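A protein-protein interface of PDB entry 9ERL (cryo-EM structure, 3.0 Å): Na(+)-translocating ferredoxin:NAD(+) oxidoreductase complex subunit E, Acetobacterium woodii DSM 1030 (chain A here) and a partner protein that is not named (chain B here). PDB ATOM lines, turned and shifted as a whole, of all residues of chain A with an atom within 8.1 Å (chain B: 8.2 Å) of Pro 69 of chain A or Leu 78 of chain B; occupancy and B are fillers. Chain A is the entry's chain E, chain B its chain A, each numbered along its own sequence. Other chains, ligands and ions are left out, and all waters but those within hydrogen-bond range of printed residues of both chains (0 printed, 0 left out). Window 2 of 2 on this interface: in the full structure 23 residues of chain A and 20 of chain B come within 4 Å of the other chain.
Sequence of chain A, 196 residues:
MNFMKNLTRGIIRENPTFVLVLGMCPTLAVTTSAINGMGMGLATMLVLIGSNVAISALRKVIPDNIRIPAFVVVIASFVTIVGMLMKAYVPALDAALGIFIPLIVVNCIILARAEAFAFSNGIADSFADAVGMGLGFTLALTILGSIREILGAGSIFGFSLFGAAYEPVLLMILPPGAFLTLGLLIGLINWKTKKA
O of Asn 65 of chain A is in hydrogen-bond range of NE2 of Gln 85 of chain B (3.1 Å).
Among the printed residues, merely in contact across the chains: Ile 68 of chain A with Gln 85 of chain B (3.98 Å), Pro 69 of chain A with Leu 78 of chain B (3.9 Å), Pro 69 of chain A with Gln 85 of chain B (3.8 Å), Val 73 of chain A with Ile 74 of chain B (3.5 Å) and Ala 76 of chain A with Ile 74 of chain B (3.7 Å).
Of the printed residues of chain B, Asn 65 of chain A touches Gln 85 (3.1 Å).
Of the printed residues of chain B, Ile 68 of chain A touches Gln 85.
Of chain B, only Leu 78 and Gln 85 come within 4 Å of Pro 69 of chain A.
Of the printed residues of chain B, Val 73 of chain A touches Ile 74 (3.5 Å).
Printed residues of chain B within 4 Å of Ala 76 of chain A: Ile 74.
Of chain A, only Pro 69 comes within 4 Å of Leu 78 of chain B.
Of the printed residues of chain A, Gln 85 of chain B touches Asn 65 (3.1 Å), Ile 68 (3.98 Å) and Pro 69 (3.8 Å).
The nearest residue of chain B that does not touch Pro 69 of chain A is Ala 81 of chain B (4.5 Å).
Of the 17 printed residues of chain B, 3 touch a printed residue of chain A.
Hydrophobic or aromatic side chains of chain B that line the printed part of chain A: Ile 74 and Leu 78.
Hydrophobic or aromatic side chains of chain A within 4 Å of the printed part of chain B: Ile 68, Pro 69 and Ala 76.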
ATOM      1  N   ILE A  62     -17.175  -1.515   1.309  1.00  0.00           N
ATOM      2  CA  ILE A  62     -17.901  -0.319   1.730  1.00  0.00           C
ATOM      3  C   ILE A  62     -18.460  -0.535   3.132  1.00  0.00           C
ATOM      4  O   ILE A  62     -19.218  -1.490   3.355  1.00  0.00           O
ATOM      5  CB  ILE A  62     -19.021   0.029   0.739  1.00  0.00           C
ATOM      6  CG1 ILE A  62     -18.434   0.393  -0.626  1.00  0.00           C
ATOM      7  CG2 ILE A  62     -19.868   1.173   1.271  1.00  0.00           C
ATOM      8  CD1 ILE A  62     -19.480   0.617  -1.697  1.00  0.00           C
ATOM      9  N   PRO A  63     -18.116   0.317   4.103  1.00  0.00           N
ATOM     10  CA  PRO A  63     -18.701   0.183   5.446  1.00  0.00           C
ATOM     11  C   PRO A  63     -20.167   0.581   5.489  1.00  0.00           C
ATOM     12  O   PRO A  63     -20.737   1.008   4.480  1.00  0.00           O
ATOM     13  CB  PRO A  63     -17.839   1.126   6.299  1.00  0.00           C
ATOM     14  CG  PRO A  63     -16.585   1.332   5.504  1.00  0.00           C
ATOM     15  CD  PRO A  63     -17.029   1.306   4.078  1.00  0.00           C
ATOM     16  N   ASP A  64     -20.786   0.452   6.662  1.00  0.00           N
ATOM     17  CA  ASP A  64     -22.213   0.725   6.787  1.00  0.00           C
ATOM     18  C   ASP A  64     -22.510   2.207   6.979  1.00  0.00           C
ATOM     19  O   ASP A  64     -23.627   2.651   6.693  1.00  0.00           O
ATOM     20  CB  ASP A  64     -22.795  -0.080   7.952  1.00  0.00           C
ATOM     21  CG  ASP A  64     -24.210  -0.556   7.687  1.00  0.00           C
ATOM     22  OD1 ASP A  64     -24.981   0.182   7.040  1.00  0.00           O
ATOM     23  OD2 ASP A  64     -24.552  -1.673   8.126  1.00  0.00           O
ATOM     24  N   ASN A  65     -21.540   2.985   7.455  1.00  0.00           N
ATOM     25  CA  ASN A  65     -21.781   4.380   7.802  1.00  0.00           C
ATOM     26  C   ASN A  65     -21.554   5.352   6.649  1.00  0.00           C
ATOM     27  O   ASN A  65     -21.977   6.508   6.748  1.00  0.00           O
ATOM     28  CB  ASN A  65     -20.898   4.787   8.985  1.00  0.00           C
ATOM     29  CG  ASN A  65     -21.551   4.506  10.322  1.00  0.00           C
ATOM     30  OD1 ASN A  65     -22.777   4.517  10.441  1.00  0.00           O
ATOM     31  ND2 ASN A  65     -20.736   4.249  11.337  1.00  0.00           N
ATOM     32  N   ILE A  66     -20.905   4.925   5.567  1.00  0.00           N
ATOM     33  CA  ILE A  66     -20.619   5.823   4.453  1.00  0.00           C
ATOM     34  C   ILE A  66     -21.126   5.222   3.150  1.00  0.00           C
ATOM     35  O   ILE A  66     -20.549   5.455   2.082  1.00  0.00           O
ATOM     36  CB  ILE A  66     -19.114   6.140   4.363  1.00  0.00           C
ATOM     37  CG1 ILE A  66     -18.289   4.852   4.360  1.00  0.00           C
ATOM     38  CG2 ILE A  66     -18.689   7.046   5.507  1.00  0.00           C
ATOM     39  CD1 ILE A  66     -17.001   4.963   3.581  1.00  0.00           C
ATOM     40  N   ARG A  67     -22.202   4.437   3.226  1.00  0.00           N
ATOM     41  CA  ARG A  67     -22.740   3.799   2.027  1.00  0.00           C
ATOM     42  C   ARG A  67     -23.382   4.820   1.094  1.00  0.00           C
ATOM     43  O   ARG A  67     -23.195   4.763  -0.129  1.00  0.00           O
ATOM     44  CB  ARG A  67     -23.748   2.717   2.416  1.00  0.00           C
ATOM     45  CG  ARG A  67     -24.701   3.127   3.527  1.00  0.00           C
ATOM     46  CD  ARG A  67     -25.706   2.033   3.839  1.00  0.00           C
ATOM     47  NE  ARG A  67     -26.634   2.441   4.884  1.00  0.00           N
ATOM     48  CZ  ARG A  67     -27.946   2.552   4.719  1.00  0.00           C
ATOM     49  NH1 ARG A  67     -28.521   2.277   3.561  1.00  0.00           N
ATOM     50  NH2 ARG A  67     -28.697   2.950   5.741  1.00  0.00           N
ATOM     51  N   ILE A  68     -24.154   5.756   1.654  1.00  0.00           N
ATOM     52  CA  ILE A  68     -24.870   6.732   0.826  1.00  0.00           C
ATOM     53  C   ILE A  68     -23.931   7.636   0.028  1.00  0.00           C
ATOM     54  O   ILE A  68     -24.202   7.868  -1.162  1.00  0.00           O
ATOM     55  CB  ILE A  68     -25.873   7.520   1.678  1.00  0.00           C
ATOM     56  CG1 ILE A  68     -26.662   6.580   2.591  1.00  0.00           C
ATOM     57  CG2 ILE A  68     -26.822   8.312   0.796  1.00  0.00           C
ATOM     58  CD1 ILE A  68     -27.476   7.300   3.641  1.00  0.00           C
ATOM     59  N   PRO A  69     -22.857   8.211   0.606  1.00  0.00           N
ATOM     60  CA  PRO A  69     -21.946   9.010  -0.239  1.00  0.00           C
ATOM     61  C   PRO A  69     -21.328   8.232  -1.390  1.00  0.00           C
ATOM     62  O   PRO A  69     -21.261   8.755  -2.509  1.00  0.00           O
ATOM     63  CB  PRO A  69     -20.886   9.491   0.760  1.00  0.00           C
ATOM     64  CG  PRO A  69     -21.605   9.558   2.042  1.00  0.00           C
ATOM     65  CD  PRO A  69     -22.500   8.361   2.032  1.00  0.00           C
ATOM     66  N   ALA A  70     -20.901   6.988  -1.161  1.00  0.00           N
ATOM     67  CA  ALA A  70     -20.334   6.193  -2.247  1.00  0.00           C
ATOM     68  C   ALA A  70     -21.377   5.892  -3.317  1.00  0.00           C
ATOM     69  O   ALA A  70     -21.089   5.982  -4.522  1.00  0.00           O
ATOM     70  CB  ALA A  70     -19.742   4.898  -1.694  1.00  0.00           C
ATOM     71  N   PHE A  71     -22.595   5.547  -2.892  1.00  0.00           N
ATOM     72  CA  PHE A  71     -23.660   5.242  -3.840  1.00  0.00           C
ATOM     73  C   PHE A  71     -23.980   6.450  -4.710  1.00  0.00           C
ATOM     74  O   PHE A  71     -24.067   6.340  -5.941  1.00  0.00           O
ATOM     75  CB  PHE A  71     -24.911   4.777  -3.091  1.00  0.00           C
ATOM     76  CG  PHE A  71     -24.780   3.416  -2.457  1.00  0.00           C
ATOM     77  CD1 PHE A  71     -23.716   2.583  -2.764  1.00  0.00           C
ATOM     78  CD2 PHE A  71     -25.728   2.971  -1.551  1.00  0.00           C
ATOM     79  CE1 PHE A  71     -23.600   1.337  -2.177  1.00  0.00           C
ATOM     80  CE2 PHE A  71     -25.618   1.726  -0.963  1.00  0.00           C
ATOM     81  CZ  PHE A  71     -24.553   0.909  -1.276  1.00  0.00           C
ATOM     82  N   VAL A  72     -24.135   7.623  -4.087  1.00  0.00           N
ATOM     83  CA  VAL A  72     -24.489   8.805  -4.866  1.00  0.00           C
ATOM     84  C   VAL A  72     -23.321   9.250  -5.739  1.00  0.00           C
ATOM     85  O   VAL A  72     -23.539   9.775  -6.833  1.00  0.00           O
ATOM     86  CB  VAL A  72     -25.002   9.948  -3.964  1.00  0.00           C
ATOM     87  CG1 VAL A  72     -26.210   9.491  -3.161  1.00  0.00           C
ATOM     88  CG2 VAL A  72     -23.912  10.481  -3.054  1.00  0.00           C
ATOM     89  N   VAL A  73     -22.077   9.019  -5.307  1.00  0.00           N
ATOM     90  CA  VAL A  73     -20.931   9.354  -6.150  1.00  0.00           C
ATOM     91  C   VAL A  73     -20.936   8.510  -7.421  1.00  0.00           C
ATOM     92  O   VAL A  73     -20.781   9.035  -8.533  1.00  0.00           O
ATOM     93  CB  VAL A  73     -19.619   9.188  -5.360  1.00  0.00           C
ATOM     94  CG1 VAL A  73     -18.452   8.941  -6.301  1.00  0.00           C
ATOM     95  CG2 VAL A  73     -19.352  10.420  -4.514  1.00  0.00           C
ATOM     96  N   VAL A  74     -21.148   7.197  -7.280  1.00  0.00           N
ATOM     97  CA  VAL A  74     -21.146   6.316  -8.450  1.00  0.00           C
ATOM     98  C   VAL A  74     -22.303   6.662  -9.387  1.00  0.00           C
ATOM     99  O   VAL A  74     -22.127   6.787 -10.614  1.00  0.00           O
ATOM    100  CB  VAL A  74     -21.198   4.842  -8.009  1.00  0.00           C
ATOM    101  CG1 VAL A  74     -21.377   3.931  -9.209  1.00  0.00           C
ATOM    102  CG2 VAL A  74     -19.937   4.475  -7.243  1.00  0.00           C
ATOM    103  N   ILE A  75     -23.501   6.844  -8.820  1.00  0.00           N
ATOM    104  CA  ILE A  75     -24.675   7.142  -9.636  1.00  0.00           C
ATOM    105  C   ILE A  75     -24.508   8.478 -10.353  1.00  0.00           C
ATOM    106  O   ILE A  75     -24.848   8.608 -11.535  1.00  0.00           O
ATOM    107  CB  ILE A  75     -25.949   7.109  -8.771  1.00  0.00           C
ATOM    108  CG1 ILE A  75     -26.207   5.694  -8.256  1.00  0.00           C
ATOM    109  CG2 ILE A  75     -27.154   7.589  -9.561  1.00  0.00           C
ATOM    110  CD1 ILE A  75     -27.180   5.635  -7.099  1.00  0.00           C
ATOM    111  N   ALA A  76     -23.963   9.483  -9.661  1.00  0.00           N
ATOM    112  CA  ALA A  76     -23.785  10.794 -10.270  1.00  0.00           C
ATOM    113  C   ALA A  76     -22.728  10.764 -11.365  1.00  0.00           C
ATOM    114  O   ALA A  76     -22.858  11.470 -12.370  1.00  0.00           O
ATOM    115  CB  ALA A  76     -23.424  11.823  -9.200  1.00  0.00           C
ATOM    116  N   VAL A 105     -29.952  11.188 -11.049  1.00  0.00           N
ATOM    117  CA  VAL A 105     -29.198  10.713  -9.891  1.00  0.00           C
ATOM    118  C   VAL A 105     -30.123  10.475  -8.702  1.00  0.00           C
ATOM    119  O   VAL A 105     -29.880   9.577  -7.885  1.00  0.00           O
ATOM    120  CB  VAL A 105     -28.062  11.707  -9.560  1.00  0.00           C
ATOM    121  CG1 VAL A 105     -28.608  13.102  -9.295  1.00  0.00           C
ATOM    122  CG2 VAL A 105     -27.226  11.219  -8.385  1.00  0.00           C
ATOM    123  N   LEU A 111     -31.552   4.332  -6.182  1.00  0.00           N
ATOM    124  CA  LEU A 111     -31.071   4.222  -4.808  1.00  0.00           C
ATOM    125  C   LEU A 111     -31.856   3.177  -4.026  1.00  0.00           C
ATOM    126  O   LEU A 111     -31.295   2.491  -3.165  1.00  0.00           O
ATOM    127  CB  LEU A 111     -31.150   5.582  -4.115  1.00  0.00           C
ATOM    128  CG  LEU A 111     -30.263   5.778  -2.883  1.00  0.00           C
ATOM    129  CD1 LEU A 111     -28.830   5.369  -3.175  1.00  0.00           C
ATOM    130  CD2 LEU A 111     -30.324   7.220  -2.403  1.00  0.00           C
ATOM    131  N   LEU B  71     -18.600  19.498 -12.643  1.00  0.00           N
ATOM    132  CA  LEU B  71     -18.673  18.678 -11.442  1.00  0.00           C
ATOM    133  C   LEU B  71     -19.810  19.096 -10.521  1.00  0.00           C
ATOM    134  O   LEU B  71     -20.114  18.367  -9.568  1.00  0.00           O
ATOM    135  CB  LEU B  71     -17.348  18.732 -10.681  1.00  0.00           C
ATOM    136  CG  LEU B  71     -16.073  18.353 -11.431  1.00  0.00           C
ATOM    137  CD1 LEU B  71     -14.852  18.648 -10.580  1.00  0.00           C
ATOM    138  CD2 LEU B  71     -16.104  16.888 -11.822  1.00  0.00           C
ATOM    139  N   GLN B  72     -20.461  20.230 -10.824  1.00  0.00           N
ATOM    140  CA  GLN B  72     -21.423  20.863  -9.922  1.00  0.00           C
ATOM    141  C   GLN B  72     -22.359  19.846  -9.290  1.00  0.00           C
ATOM    142  O   GLN B  72     -22.304  19.612  -8.073  1.00  0.00           O
ATOM    143  CB  GLN B  72     -22.228  21.914 -10.685  1.00  0.00           C
ATOM    144  CG  GLN B  72     -23.043  22.841  -9.807  1.00  0.00           C
ATOM    145  CD  GLN B  72     -24.085  23.616 -10.588  1.00  0.00           C
ATOM    146  OE1 GLN B  72     -24.145  24.842 -10.522  1.00  0.00           O
ATOM    147  NE2 GLN B  72     -24.920  22.899 -11.330  1.00  0.00           N
ATOM    148  N   THR B  73     -23.132  19.146 -10.129  1.00  0.00           N
ATOM    149  CA  THR B  73     -24.149  18.221  -9.643  1.00  0.00           C
ATOM    150  C   THR B  73     -23.569  17.222  -8.654  1.00  0.00           C
ATOM    151  O   THR B  73     -24.034  17.149  -7.508  1.00  0.00           O
ATOM    152  CB  THR B  73     -24.800  17.488 -10.816  1.00  0.00           C
ATOM    153  OG1 THR B  73     -25.605  18.402 -11.569  1.00  0.00           O
ATOM    154  CG2 THR B  73     -25.673  16.350 -10.313  1.00  0.00           C
ATOM    155  N   ILE B  74     -22.491  16.522  -9.034  1.00  0.00           N
ATOM    156  CA  ILE B  74     -21.995  15.477  -8.141  1.00  0.00           C
ATOM    157  C   ILE B  74     -21.509  16.099  -6.843  1.00  0.00           C
ATOM    158  O   ILE B  74     -21.897  15.651  -5.753  1.00  0.00           O
ATOM    159  CB  ILE B  74     -20.927  14.586  -8.818  1.00  0.00           C
ATOM    160  CG1 ILE B  74     -20.462  13.487  -7.862  1.00  0.00           C
ATOM    161  CG2 ILE B  74     -19.727  15.352  -9.322  1.00  0.00           C
ATOM    162  CD1 ILE B  74     -19.679  12.387  -8.540  1.00  0.00           C
ATOM    163  N   ALA B  75     -20.786  17.224  -6.936  1.00  0.00           N
ATOM    164  CA  ALA B  75     -20.333  17.898  -5.727  1.00  0.00           C
ATOM    165  C   ALA B  75     -21.517  18.244  -4.846  1.00  0.00           C
ATOM    166  O   ALA B  75     -21.544  17.873  -3.663  1.00  0.00           O
ATOM    167  CB  ALA B  75     -19.535  19.149  -6.085  1.00  0.00           C
ATOM    168  N   PHE B  76     -22.563  18.818  -5.454  1.00  0.00           N
ATOM    169  CA  PHE B  76     -23.738  19.210  -4.692  1.00  0.00           C
ATOM    170  C   PHE B  76     -24.315  18.018  -3.952  1.00  0.00           C
ATOM    171  O   PHE B  76     -24.474  18.063  -2.722  1.00  0.00           O
ATOM    172  CB  PHE B  76     -24.789  19.831  -5.615  1.00  0.00           C
ATOM    173  CG  PHE B  76     -24.554  21.287  -5.922  1.00  0.00           C
ATOM    174  CD1 PHE B  76     -23.327  21.882  -5.676  1.00  0.00           C
ATOM    175  CD2 PHE B  76     -25.570  22.063  -6.455  1.00  0.00           C
ATOM    176  CE1 PHE B  76     -23.118  23.217  -5.960  1.00  0.00           C
ATOM    177  CE2 PHE B  76     -25.366  23.398  -6.737  1.00  0.00           C
ATOM    178  CZ  PHE B  76     -24.139  23.975  -6.489  1.00  0.00           C
ATOM    179  N   ILE B  77     -24.508  16.896  -4.660  1.00  0.00           N
ATOM    180  CA  ILE B  77     -25.224  15.795  -4.030  1.00  0.00           C
ATOM    181  C   ILE B  77     -24.399  15.246  -2.883  1.00  0.00           C
ATOM    182  O   ILE B  77     -24.956  14.901  -1.829  1.00  0.00           O
ATOM    183  CB  ILE B  77     -25.631  14.713  -5.055  1.00  0.00           C
ATOM    184  CG1 ILE B  77     -26.753  13.839  -4.488  1.00  0.00           C
ATOM    185  CG2 ILE B  77     -24.466  13.836  -5.476  1.00  0.00           C
ATOM    186  CD1 ILE B  77     -27.982  14.608  -4.072  1.00  0.00           C
ATOM    187  N   LEU B  78     -23.063  15.293  -3.012  1.00  0.00           N
ATOM    188  CA  LEU B  78     -22.200  14.799  -1.947  1.00  0.00           C
ATOM    189  C   LEU B  78     -22.517  15.510  -0.646  1.00  0.00           C
ATOM    190  O   LEU B  78     -22.862  14.865   0.356  1.00  0.00           O
ATOM    191  CB  LEU B  78     -20.730  14.987  -2.328  1.00  0.00           C
ATOM    192  CG  LEU B  78     -19.692  14.176  -1.550  1.00  0.00           C
ATOM    193  CD1 LEU B  78     -20.176  12.757  -1.302  1.00  0.00           C
ATOM    194  CD2 LEU B  78     -18.359  14.168  -2.281  1.00  0.00           C
ATOM    195  N   ILE B  79     -22.552  16.848  -0.692  1.00  0.00           N
ATOM    196  CA  ILE B  79     -22.818  17.624   0.514  1.00  0.00           C
ATOM    197  C   ILE B  79     -24.161  17.226   1.095  1.00  0.00           C
ATOM    198  O   ILE B  79     -24.257  16.864   2.279  1.00  0.00           O
ATOM    199  CB  ILE B  79     -22.753  19.132   0.206  1.00  0.00           C
ATOM    200  CG1 ILE B  79     -21.299  19.578   0.036  1.00  0.00           C
ATOM    201  CG2 ILE B  79     -23.433  19.934   1.302  1.00  0.00           C
ATOM    202  CD1 ILE B  79     -21.110  20.640  -1.020  1.00  0.00           C
ATOM    203  N   ILE B  80     -25.186  17.150   0.237  1.00  0.00           N
ATOM    204  CA  ILE B  80     -26.531  16.872   0.721  1.00  0.00           C
ATOM    205  C   ILE B  80     -26.557  15.526   1.418  1.00  0.00           C
ATOM    206  O   ILE B  80     -27.094  15.403   2.530  1.00  0.00           O
ATOM    207  CB  ILE B  80     -27.547  16.946  -0.433  1.00  0.00           C
ATOM    208  CG1 ILE B  80     -27.828  18.404  -0.799  1.00  0.00           C
ATOM    209  CG2 ILE B  80     -28.843  16.244  -0.058  1.00  0.00           C
ATOM    210  CD1 ILE B  80     -28.128  18.620  -2.264  1.00  0.00           C
ATOM    211  N   ALA B  81     -25.871  14.531   0.835  1.00  0.00           N
ATOM    212  CA  ALA B  81     -25.871  13.197   1.416  1.00  0.00           C
ATOM    213  C   ALA B  81     -25.369  13.240   2.847  1.00  0.00           C
ATOM    214  O   ALA B  81     -26.062  12.779   3.766  1.00  0.00           O
ATOM    215  CB  ALA B  81     -25.021  12.250   0.571  1.00  0.00           C
ATOM    216  N   ALA B  82     -24.232  13.915   3.066  1.00  0.00           N
ATOM    217  CA  ALA B  82     -23.669  13.980   4.408  1.00  0.00           C
ATOM    218  C   ALA B  82     -24.659  14.615   5.369  1.00  0.00           C
ATOM    219  O   ALA B  82     -24.936  14.057   6.441  1.00  0.00           O
ATOM    220  CB  ALA B  82     -22.353  14.754   4.393  1.00  0.00           C
ATOM    221  N   LEU B  83     -25.289  15.717   4.944  1.00  0.00           N
ATOM    222  CA  LEU B  83     -26.245  16.397   5.807  1.00  0.00           C
ATOM    223  C   LEU B  83     -27.376  15.462   6.192  1.00  0.00           C
ATOM    224  O   LEU B  83     -27.703  15.328   7.380  1.00  0.00           O
ATOM    225  CB  LEU B  83     -26.793  17.644   5.113  1.00  0.00           C
ATOM    226  CG  LEU B  83     -26.296  19.004   5.605  1.00  0.00           C
ATOM    227  CD1 LEU B  83     -24.779  19.082   5.545  1.00  0.00           C
ATOM    228  CD2 LEU B  83     -26.925  20.119   4.791  1.00  0.00           C
ATOM    229  N   VAL B  84     -27.913  14.729   5.212  1.00  0.00           N
ATOM    230  CA  VAL B  84     -29.032  13.844   5.501  1.00  0.00           C
ATOM    231  C   VAL B  84     -28.596  12.759   6.471  1.00  0.00           C
ATOM    232  O   VAL B  84     -29.326  12.426   7.415  1.00  0.00           O
ATOM    233  CB  VAL B  84     -29.607  13.262   4.200  1.00  0.00           C
ATOM    234  CG1 VAL B  84     -30.654  12.202   4.501  1.00  0.00           C
ATOM    235  CG2 VAL B  84     -30.203  14.375   3.357  1.00  0.00           C
ATOM    236  N   GLN B  85     -27.366  12.257   6.303  1.00  0.00           N
ATOM    237  CA  GLN B  85     -26.856  11.253   7.226  1.00  0.00           C
ATOM    238  C   GLN B  85     -26.845  11.798   8.644  1.00  0.00           C
ATOM    239  O   GLN B  85     -27.338  11.141   9.571  1.00  0.00           O
ATOM    240  CB  GLN B  85     -25.456  10.809   6.805  1.00  0.00           C
ATOM    241  CG  GLN B  85     -24.961   9.562   7.514  1.00  0.00           C
ATOM    242  CD  GLN B  85     -24.672   8.427   6.556  1.00  0.00           C
ATOM    243  OE1 GLN B  85     -24.196   8.647   5.443  1.00  0.00           O
ATOM    244  NE2 GLN B  85     -24.957   7.203   6.983  1.00  0.00           N
ATOM    245  N   THR B 110     -32.359  12.710   0.637  1.00  0.00           N
ATOM    246  CA  THR B 110     -31.443  13.112  -0.427  1.00  0.00           C
ATOM    247  C   THR B 110     -32.124  13.070  -1.787  1.00  0.00           C
ATOM    248  O   THR B 110     -31.775  13.844  -2.685  1.00  0.00           O
ATOM    249  CB  THR B 110     -30.219  12.198  -0.459  1.00  0.00           C
ATOM    250  OG1 THR B 110     -30.494  11.069  -1.296  1.00  0.00           O
ATOM    251  CG2 THR B 110     -29.893  11.688   0.921  1.00  0.00           C
ATOM    252  N   LEU B 116     -32.041  19.439  -4.054  1.00  0.00           N
ATOM    253  CA  LEU B 116     -31.188  19.652  -5.218  1.00  0.00           C
ATOM    254  C   LEU B 116     -31.877  20.535  -6.248  1.00  0.00           C
ATOM    255  O   LEU B 116     -31.226  21.349  -6.915  1.00  0.00           O
ATOM    256  CB  LEU B 116     -30.799  18.308  -5.834  1.00  0.00           C
ATOM    257  CG  LEU B 116     -29.661  18.317  -6.857  1.00  0.00           C
ATOM    258  CD1 LEU B 116     -28.403  18.919  -6.258  1.00  0.00           C
ATOM    259  CD2 LEU B 116     -29.392  16.913  -7.372  1.00  0.00           C
